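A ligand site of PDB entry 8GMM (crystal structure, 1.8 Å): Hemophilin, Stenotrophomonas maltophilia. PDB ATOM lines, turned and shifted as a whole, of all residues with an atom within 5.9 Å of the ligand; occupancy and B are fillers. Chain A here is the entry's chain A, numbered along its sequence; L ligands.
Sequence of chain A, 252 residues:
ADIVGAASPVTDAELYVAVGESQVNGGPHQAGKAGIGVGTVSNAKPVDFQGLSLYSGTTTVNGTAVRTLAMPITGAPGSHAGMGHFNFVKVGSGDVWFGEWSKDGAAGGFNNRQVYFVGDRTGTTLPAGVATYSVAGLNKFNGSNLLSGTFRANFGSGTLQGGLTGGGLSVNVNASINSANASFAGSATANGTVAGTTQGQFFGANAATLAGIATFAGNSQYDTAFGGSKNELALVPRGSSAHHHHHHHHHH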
ATOM      1  N   VAL A  24       9.585  -2.260   0.621  1.00  0.00           N
ATOM      2  CA  VAL A  24       8.895  -1.090   1.130  1.00  0.00           C
ATOM      3  C   VAL A  24       7.804  -0.685   0.147  1.00  0.00           C
ATOM      4  O   VAL A  24       8.082  -0.421  -1.032  1.00  0.00           O
ATOM      5  CB  VAL A  24       9.887   0.058   1.367  1.00  0.00           C
ATOM      6  CG1 VAL A  24       9.153   1.314   1.826  1.00  0.00           C
ATOM      7  CG2 VAL A  24      10.962  -0.368   2.382  1.00  0.00           C
ATOM      8  N   GLY A  26       5.710   2.409   0.186  1.00  0.00           N
ATOM      9  CA  GLY A  26       5.517   3.704   0.800  1.00  0.00           C
ATOM     10  C   GLY A  26       6.299   4.779   0.053  1.00  0.00           C
ATOM     11  O   GLY A  26       7.330   4.462  -0.534  1.00  0.00           O
ATOM     12  N   GLY A  27       5.809   6.019   0.043  1.00  0.00           N
ATOM     13  CA  GLY A  27       6.453   7.058  -0.742  1.00  0.00           C
ATOM     14  C   GLY A  27       6.570   6.636  -2.206  1.00  0.00           C
ATOM     15  O   GLY A  27       5.595   6.183  -2.814  1.00  0.00           O
ATOM     16  N   PRO A  28       7.741   6.824  -2.808  1.00  0.00           N
ATOM     17  CA  PRO A  28       7.951   6.361  -4.194  1.00  0.00           C
ATOM     18  C   PRO A  28       8.296   4.885  -4.298  1.00  0.00           C
ATOM     19  O   PRO A  28       8.525   4.391  -5.420  1.00  0.00           O
ATOM     20  CB  PRO A  28       9.129   7.216  -4.660  1.00  0.00           C
ATOM     21  CG  PRO A  28       9.954   7.391  -3.400  1.00  0.00           C
ATOM     22  CD  PRO A  28       8.962   7.471  -2.267  1.00  0.00           C
ATOM     23  N   HIS A  29       8.349   4.163  -3.193  1.00  0.00           N
ATOM     24  CA  HIS A  29       8.901   2.818  -3.180  1.00  0.00           C
ATOM     25  C   HIS A  29       7.800   1.783  -3.387  1.00  0.00           C
ATOM     26  O   HIS A  29       6.697   1.910  -2.828  1.00  0.00           O
ATOM     27  CB  HIS A  29       9.588   2.552  -1.851  1.00  0.00           C
ATOM     28  CG  HIS A  29      10.579   3.582  -1.465  1.00  0.00           C
ATOM     29  ND1 HIS A  29      11.639   3.954  -2.284  1.00  0.00           N
ATOM     30  CD2 HIS A  29      10.698   4.345  -0.355  1.00  0.00           C
ATOM     31  CE1 HIS A  29      12.357   4.883  -1.683  1.00  0.00           C
ATOM     32  NE2 HIS A  29      11.803   5.143  -0.519  1.00  0.00           N
ATOM     33  N   ILE A  36      17.616  -2.211  -2.940  1.00  0.00           N
ATOM     34  CA  ILE A  36      18.763  -1.990  -2.065  1.00  0.00           C
ATOM     35  C   ILE A  36      18.279  -1.345  -0.769  1.00  0.00           C
ATOM     36  O   ILE A  36      17.349  -0.522  -0.764  1.00  0.00           O
ATOM     37  CB  ILE A  36      19.819  -1.116  -2.772  1.00  0.00           C
ATOM     38  CG1 ILE A  36      21.092  -1.045  -1.943  1.00  0.00           C
ATOM     39  CG2 ILE A  36      19.281   0.284  -3.065  1.00  0.00           C
ATOM     40  CD1 ILE A  36      22.295  -0.639  -2.759  1.00  0.00           C
ATOM     41  N   GLY A  37      18.924  -1.721   0.328  1.00  0.00           N
ATOM     42  CA  GLY A  37      18.689  -1.090   1.607  1.00  0.00           C
ATOM     43  C   GLY A  37      20.015  -0.603   2.161  1.00  0.00           C
ATOM     44  O   GLY A  37      21.077  -1.121   1.829  1.00  0.00           O
ATOM     45  N   VAL A  38      19.931   0.431   2.997  1.00  0.00           N
ATOM     46  CA  VAL A  38      21.098   1.005   3.665  1.00  0.00           C
ATOM     47  C   VAL A  38      20.876   0.915   5.167  1.00  0.00           C
ATOM     48  O   VAL A  38      19.756   1.145   5.652  1.00  0.00           O
ATOM     49  CB  VAL A  38      21.361   2.451   3.197  1.00  0.00           C
ATOM     50  CG1 VAL A  38      20.230   3.381   3.634  1.00  0.00           C
ATOM     51  CG2 VAL A  38      22.710   2.947   3.693  1.00  0.00           C
ATOM     52  N   VAL A  41      18.822   3.443   7.389  1.00  0.00           N
ATOM     53  CA  VAL A  41      17.401   3.709   7.193  1.00  0.00           C
ATOM     54  C   VAL A  41      16.682   2.388   7.400  1.00  0.00           C
ATOM     55  O   VAL A  41      16.766   1.483   6.565  1.00  0.00           O
ATOM     56  CB  VAL A  41      17.101   4.279   5.803  1.00  0.00           C
ATOM     57  CG1 VAL A  41      15.611   4.670   5.686  1.00  0.00           C
ATOM     58  CG2 VAL A  41      17.999   5.471   5.517  1.00  0.00           C
ATOM     59  N   SER A  42      15.999   2.274   8.538  1.00  0.00           N
ATOM     60  CA  SER A  42      15.198   1.106   8.893  1.00  0.00           C
ATOM     61  C   SER A  42      15.985  -0.187   8.733  1.00  0.00           C
ATOM     62  O   SER A  42      15.512  -1.165   8.150  1.00  0.00           O
ATOM     63  CB  SER A  42      13.910   1.088   8.063  1.00  0.00           C
ATOM     64  OG  SER A  42      12.888   0.375   8.729  1.00  0.00           O
ATOM     65  N   ALA A  44      18.261  -1.255   6.859  1.00  0.00           N
ATOM     66  CA  ALA A  44      18.501  -1.728   5.504  1.00  0.00           C
ATOM     67  C   ALA A  44      17.306  -2.444   4.887  1.00  0.00           C
ATOM     68  O   ALA A  44      17.472  -3.249   3.958  1.00  0.00           O
ATOM     69  CB  ALA A  44      19.740  -2.636   5.458  1.00  0.00           C
ATOM     70  N   LYS A  45      16.091  -2.144   5.318  1.00  0.00           N
ATOM     71  CA  LYS A  45      14.939  -2.641   4.587  1.00  0.00           C
ATOM     72  C   LYS A  45      15.028  -2.133   3.145  1.00  0.00           C
ATOM     73  O   LYS A  45      15.226  -0.925   2.938  1.00  0.00           O
ATOM     74  CB  LYS A  45      13.631  -2.185   5.235  1.00  0.00           C
ATOM     75  CG  LYS A  45      12.431  -2.922   4.672  1.00  0.00           C
ATOM     76  CD  LYS A  45      11.134  -2.575   5.388  1.00  0.00           C
ATOM     77  CE  LYS A  45       9.986  -3.461   4.906  1.00  0.00           C
ATOM     78  NZ  LYS A  45       8.696  -3.166   5.580  1.00  0.00           N
ATOM     79  N   PRO A  46      14.972  -2.998   2.131  1.00  0.00           N
ATOM     80  CA  PRO A  46      15.306  -2.552   0.780  1.00  0.00           C
ATOM     81  C   PRO A  46      14.152  -1.887   0.041  1.00  0.00           C
ATOM     82  O   PRO A  46      12.983  -2.253   0.178  1.00  0.00           O
ATOM     83  CB  PRO A  46      15.748  -3.858   0.083  1.00  0.00           C
ATOM     84  CG  PRO A  46      15.018  -4.933   0.817  1.00  0.00           C
ATOM     85  CD  PRO A  46      14.854  -4.469   2.224  1.00  0.00           C
ATOM     86  N   VAL A  47      14.521  -0.889  -0.768  1.00  0.00           N
ATOM     87  CA  VAL A  47      13.608  -0.188  -1.654  1.00  0.00           C
ATOM     88  C   VAL A  47      14.076  -0.443  -3.078  1.00  0.00           C
ATOM     89  O   VAL A  47      15.203  -0.871  -3.323  1.00  0.00           O
ATOM     90  CB  VAL A  47      13.551   1.335  -1.383  1.00  0.00           C
ATOM     91  CG1 VAL A  47      13.076   1.611   0.044  1.00  0.00           C
ATOM     92  CG2 VAL A  47      14.898   1.996  -1.659  1.00  0.00           C
ATOM     93  N   LEU A  52      13.775   5.026  -7.404  1.00  0.00           N
ATOM     94  CA  LEU A  52      14.802   6.042  -7.195  1.00  0.00           C
ATOM     95  C   LEU A  52      15.098   6.842  -8.468  1.00  0.00           C
ATOM     96  O   LEU A  52      15.648   7.938  -8.382  1.00  0.00           O
ATOM     97  CB  LEU A  52      16.105   5.399  -6.717  1.00  0.00           C
ATOM     98  CG  LEU A  52      16.011   4.464  -5.508  1.00  0.00           C
ATOM     99  CD1 LEU A  52      17.387   3.891  -5.184  1.00  0.00           C
ATOM    100  CD2 LEU A  52      15.398   5.146  -4.304  1.00  0.00           C
ATOM    101  N   TYR A  55      14.227  10.559  -9.036  1.00  0.00           N
ATOM    102  CA  TYR A  55      14.813  11.461  -8.060  1.00  0.00           C
ATOM    103  C   TYR A  55      16.329  11.563  -8.180  1.00  0.00           C
ATOM    104  O   TYR A  55      16.924  12.385  -7.492  1.00  0.00           O
ATOM    105  CB  TYR A  55      14.468  10.991  -6.647  1.00  0.00           C
ATOM    106  CG  TYR A  55      12.988  11.025  -6.341  1.00  0.00           C
ATOM    107  CD1 TYR A  55      12.403  12.163  -5.833  1.00  0.00           C
ATOM    108  CD2 TYR A  55      12.179   9.917  -6.584  1.00  0.00           C
ATOM    109  CE1 TYR A  55      11.054  12.216  -5.565  1.00  0.00           C
ATOM    110  CE2 TYR A  55      10.819   9.962  -6.314  1.00  0.00           C
ATOM    111  CZ  TYR A  55      10.262  11.112  -5.794  1.00  0.00           C
ATOM    112  OH  TYR A  55       8.913  11.178  -5.520  1.00  0.00           O
ATOM    113  N   LEU A  69      22.622   9.600  -6.595  1.00  0.00           N
ATOM    114  CA  LEU A  69      21.604   9.894  -5.590  1.00  0.00           C
ATOM    115  C   LEU A  69      22.269  10.137  -4.249  1.00  0.00           C
ATOM    116  O   LEU A  69      23.054   9.318  -3.782  1.00  0.00           O
ATOM    117  CB  LEU A  69      20.594   8.751  -5.485  1.00  0.00           C
ATOM    118  CG  LEU A  69      19.410   8.994  -4.544  1.00  0.00           C
ATOM    119  CD1 LEU A  69      18.565  10.144  -5.050  1.00  0.00           C
ATOM    120  CD2 LEU A  69      18.573   7.740  -4.384  1.00  0.00           C
ATOM    121  N   MET A  71      21.430  12.930  -0.521  1.00  0.00           N
ATOM    122  CA  MET A  71      20.691  14.024   0.064  1.00  0.00           C
ATOM    123  C   MET A  71      21.346  15.360  -0.290  1.00  0.00           C
ATOM    124  O   MET A  71      22.569  15.409  -0.504  1.00  0.00           O
ATOM    125  CB  MET A  71      20.645  13.869   1.578  1.00  0.00           C
ATOM    126  CG  MET A  71      19.718  12.793   2.074  1.00  0.00           C
ATOM    127  SD  MET A  71      18.022  13.288   1.782  1.00  0.00           S
ATOM    128  CE  MET A  71      17.356  11.809   1.098  1.00  0.00           C
ATOM    129  N   ILE A  73      17.052  15.803  -0.928  1.00  0.00           N
ATOM    130  CA  ILE A  73      16.049  15.466  -1.941  1.00  0.00           C
ATOM    131  C   ILE A  73      14.694  15.957  -1.471  1.00  0.00           C
ATOM    132  O   ILE A  73      14.230  15.570  -0.388  1.00  0.00           O
ATOM    133  CB  ILE A  73      16.026  13.947  -2.191  1.00  0.00           C
ATOM    134  CG1 ILE A  73      17.361  13.523  -2.780  1.00  0.00           C
ATOM    135  CG2 ILE A  73      14.869  13.568  -3.113  1.00  0.00           C
ATOM    136  CD1 ILE A  73      17.600  12.076  -2.674  1.00  0.00           C
ATOM    137  N   THR A  74      14.041  16.800  -2.263  1.00  0.00           N
ATOM    138  CA  THR A  74      12.719  17.298  -1.908  1.00  0.00           C
ATOM    139  C   THR A  74      11.756  16.140  -1.657  1.00  0.00           C
ATOM    140  O   THR A  74      11.585  15.263  -2.513  1.00  0.00           O
ATOM    141  CB  THR A  74      12.173  18.227  -2.993  1.00  0.00           C
ATOM    142  OG1 THR A  74      13.003  19.385  -3.080  1.00  0.00           O
ATOM    143  CG2 THR A  74      10.750  18.666  -2.672  1.00  0.00           C
ATOM    144  N   GLY A  75      11.144  16.127  -0.478  1.00  0.00           N
ATOM    145  CA  GLY A  75      10.168  15.133  -0.103  1.00  0.00           C
ATOM    146  C   GLY A  75      10.727  13.904   0.579  1.00  0.00           C
ATOM    147  O   GLY A  75       9.950  12.997   0.927  1.00  0.00           O
ATOM    148  N   ALA A  76      12.053  13.838   0.799  1.00  0.00           N
ATOM    149  CA  ALA A  76      12.627  12.684   1.483  1.00  0.00           C
ATOM    150  C   ALA A  76      12.503  12.877   2.991  1.00  0.00           C
ATOM    151  O   ALA A  76      12.834  13.937   3.503  1.00  0.00           O
ATOM    152  CB  ALA A  76      14.091  12.500   1.115  1.00  0.00           C
ATOM    153  N   PRO A  77      12.054  11.856   3.732  1.00  0.00           N
ATOM    154  CA  PRO A  77      11.891  12.021   5.187  1.00  0.00           C
ATOM    155  C   PRO A  77      13.216  12.251   5.883  1.00  0.00           C
ATOM    156  O   PRO A  77      14.289  11.882   5.398  1.00  0.00           O
ATOM    157  CB  PRO A  77      11.264  10.684   5.627  1.00  0.00           C
ATOM    158  CG  PRO A  77      10.753  10.055   4.399  1.00  0.00           C
ATOM    159  CD  PRO A  77      11.624  10.524   3.284  1.00  0.00           C
ATOM    160  N   SER A  79      14.302  10.695   8.275  1.00  0.00           N
ATOM    161  CA  SER A  79      14.922   9.402   8.516  1.00  0.00           C
ATOM    162  C   SER A  79      15.953   9.073   7.466  1.00  0.00           C
ATOM    163  O   SER A  79      16.788   8.186   7.679  1.00  0.00           O
ATOM    164  CB  SER A  79      13.852   8.318   8.561  1.00  0.00           C
ATOM    165  OG  SER A  79      13.206   8.153   7.294  1.00  0.00           O
ATOM    166  N   HIS A  80      15.925   9.757   6.324  1.00  0.00           N
ATOM    167  CA  HIS A  80      16.822   9.466   5.217  1.00  0.00           C
ATOM    168  C   HIS A  80      18.112  10.265   5.270  1.00  0.00           C
ATOM    169  O   HIS A  80      18.901  10.185   4.314  1.00  0.00           O
ATOM    170  CB  HIS A  80      16.128   9.754   3.891  1.00  0.00           C
ATOM    171  CG  HIS A  80      15.018   8.810   3.584  1.00  0.00           C
ATOM    172  ND1 HIS A  80      14.098   8.403   4.531  1.00  0.00           N
ATOM    173  CD2 HIS A  80      14.681   8.164   2.439  1.00  0.00           C
ATOM    174  CE1 HIS A  80      13.250   7.558   3.974  1.00  0.00           C
ATOM    175  NE2 HIS A  80      13.592   7.399   2.720  1.00  0.00           N
ATOM    176  N   MET A  83      21.389   8.453   4.302  1.00  0.00           N
ATOM    177  CA  MET A  83      21.287   7.434   3.269  1.00  0.00           C
ATOM    178  C   MET A  83      22.596   7.220   2.525  1.00  0.00           C
ATOM    179  O   MET A  83      22.791   6.148   1.940  1.00  0.00           O
ATOM    180  CB  MET A  83      20.192   7.781   2.260  1.00  0.00           C
ATOM    181  CG  MET A  83      20.459   9.029   1.438  1.00  0.00           C
ATOM    182  SD  MET A  83      19.514   9.107  -0.121  1.00  0.00           S
ATOM    183  CE  MET A  83      17.869   8.631   0.431  1.00  0.00           C
ATOM    184  N   PHE A  86      24.887   7.072  -3.731  1.00  0.00           N
ATOM    185  CA  PHE A  86      24.737   5.957  -4.655  1.00  0.00           C
ATOM    186  C   PHE A  86      25.141   6.397  -6.062  1.00  0.00           C
ATOM    187  O   PHE A  86      24.739   7.465  -6.523  1.00  0.00           O
ATOM    188  CB  PHE A  86      23.297   5.449  -4.713  1.00  0.00           C
ATOM    189  CG  PHE A  86      22.743   4.995  -3.383  1.00  0.00           C
ATOM    190  CD1 PHE A  86      22.341   5.902  -2.429  1.00  0.00           C
ATOM    191  CD2 PHE A  86      22.591   3.642  -3.109  1.00  0.00           C
ATOM    192  CE1 PHE A  86      21.821   5.479  -1.218  1.00  0.00           C
ATOM    193  CE2 PHE A  86      22.059   3.224  -1.893  1.00  0.00           C
ATOM    194  CZ  PHE A  86      21.679   4.146  -0.955  1.00  0.00           C
HETATM  195 FE1  LIG L   1      12.612   6.247   1.165  1.00  0.00          FE
HETATM  196  C1  LIG L   1      10.143   5.424   3.349  1.00  0.00           C
HETATM  197  C2  LIG L   1      14.637   3.812   2.408  1.00  0.00           C
HETATM  198  C3  LIG L   1      15.112   7.136  -1.074  1.00  0.00           C
HETATM  199  C4  LIG L   1      10.869   9.113   0.269  1.00  0.00           C
HETATM  200  N1  LIG L   1      12.452   4.921   2.637  1.00  0.00           N
HETATM  201  C5  LIG L   1      11.290   4.669   3.350  1.00  0.00           C
HETATM  202  C6  LIG L   1      11.518   3.467   4.125  1.00  0.00           C
HETATM  203  C7  LIG L   1      12.756   3.020   3.862  1.00  0.00           C
HETATM  204  C8  LIG L   1      13.366   3.928   2.918  1.00  0.00           C
HETATM  205  C9  LIG L   1      13.450   1.763   4.434  1.00  0.00           C
HETATM  206  C10 LIG L   1      10.463   2.848   5.055  1.00  0.00           C
HETATM  207  C11 LIG L   1      10.961   2.951   6.489  1.00  0.00           C
HETATM  208  C12 LIG L   1       9.929   2.348   7.402  1.00  0.00           C
HETATM  209  O1  LIG L   1      10.288   1.473   8.226  1.00  0.00           O
HETATM  210  O2  LIG L   1       8.733   2.740   7.295  1.00  0.00           O
HETATM  211  N2  LIG L   1      14.540   5.598   0.753  1.00  0.00           N
HETATM  212  C13 LIG L   1      15.156   4.529   1.358  1.00  0.00           C
HETATM  213  C14 LIG L   1      16.431   4.316   0.707  1.00  0.00           C
HETATM  214  C15 LIG L   1      16.565   5.260  -0.246  1.00  0.00           C
HETATM  215  C16 LIG L   1      15.370   6.069  -0.234  1.00  0.00           C
HETATM  216  C17 LIG L   1      17.407   3.204   1.129  1.00  0.00           C
HETATM  217  C18 LIG L   1      17.693   5.523  -1.269  1.00  0.00           C
HETATM  218  C19 LIG L   1      18.609   4.619  -1.618  1.00  0.00           C
HETATM  219  N3  LIG L   1      12.943   7.865  -0.125  1.00  0.00           N
HETATM  220  C20 LIG L   1      14.003   7.958  -1.006  1.00  0.00           C
HETATM  221  C21 LIG L   1      13.760   9.095  -1.871  1.00  0.00           C
HETATM  222  C22 LIG L   1      12.598   9.654  -1.518  1.00  0.00           C
HETATM  223  C23 LIG L   1      12.046   8.883  -0.409  1.00  0.00           C
HETATM  224  C24 LIG L   1      14.706   9.555  -3.013  1.00  0.00           C
HETATM  225  C25 LIG L   1      12.021  10.902  -2.231  1.00  0.00           C
HETATM  226  C26 LIG L   1      10.908  11.536  -1.890  1.00  0.00           C
HETATM  227  N4  LIG L   1      10.870   7.131   1.734  1.00  0.00           N
HETATM  228  C27 LIG L   1      10.297   8.269   1.188  1.00  0.00           C
HETATM  229  C28 LIG L   1       8.968   8.413   1.757  1.00  0.00           C
HETATM  230  C29 LIG L   1       8.761   7.394   2.600  1.00  0.00           C
HETATM  231  C30 LIG L   1       9.952   6.558   2.600  1.00  0.00           C
HETATM  232  C31 LIG L   1       7.995   9.566   1.408  1.00  0.00           C
HETATM  233  C32 LIG L   1       7.501   7.115   3.453  1.00  0.00           C
HETATM  234  C33 LIG L   1       7.899   7.272   4.913  1.00  0.00           C
HETATM  235  C34 LIG L   1       6.885   8.151   5.574  1.00  0.00           C
HETATM  236  O3  LIG L   1       7.311   9.162   6.188  1.00  0.00           O
HETATM  237  O4  LIG L   1       5.667   7.845   5.450  1.00  0.00           O
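A ring nitrogen (NE2) of His 80 binds an iron atom (FE1) of the ligand (2.2 Å).
NE2 of His 29 binds FE1 of the ligand, at 2.2 Å.
The side-chain hydroxyl (OG) of Ser 42 sits at hydrogen-bond distance from an oxygen (O1) of the ligand (2.9 Å).
O of Leu 69 sits at hydrogen-bond distance from N of Phe 86 (2.9 Å).
O of Val 47 sits at hydrogen-bond distance from N of Ile 36 (2.8 Å).
The backbone NH (N) of Val 24 lies within hydrogen-bond range of the backbone carbonyl oxygen (O) of Pro 46 (3.4 Å).
A ring nitrogen (ND1) of His 80 lies within hydrogen-bond range of the side-chain hydroxyl (OG) of Ser 79, at 2.9 Å.
The backbone carbonyl oxygen (O) of Val 38 is in hydrogen-bond range of the backbone NH (N) of Ala 44 (3.1 Å).
Val 24 touches the ligand.
CA of Gly 27 touches C31 of the ligand (3.6 Å).
Pro 28 touches the ligand (CD to C4, 3.6 Å).
CG1 of Val 38 touches C17 of the ligand, 3.8 Å away.
Val 41 touches the ligand.
Lys 45 touches the ligand.
Val 47 touches the ligand (CG1 to C2, 3.6 Å).
Leu 52 touches the ligand.
CE1 of Tyr 55 touches C25 of the ligand, 3.7 Å away.
CD2 of Leu 69 touches C18 of the ligand, 3.9 Å away.
CD1 of Ile 73 touches C24 of the ligand, at 3.9 Å.
Thr 74 touches the ligand (O to C26, 3.8 Å).
Gly 75 touches the ligand.
Ala 76 touches the ligand.
Pro 77 touches the ligand (CD to C27, 3.4 Å).
Met 83 touches the ligand.
CZ of Phe 86 touches C19 of the ligand, 3.2 Å away.
Hydrophobic or aromatic side chains that line the ligand: Val 24, Pro 28, His 29, Val 38, Val 41, Val 47, Leu 52, Tyr 55, Leu 69, Ile 73, Pro 77, His 80, Met 83 and Phe 86.
20 residues have an atom within 4 Å of the ligand: Val 24, Gly 27, Pro 28, His 29, Val 38, Val 41, Ser 42, Lys 45, Val 47, Leu 52, Tyr 55, Leu 69, Ile 73, Thr 74, Gly 75, Ala 76, Pro 77, His 80, Met 83 and Phe 86.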
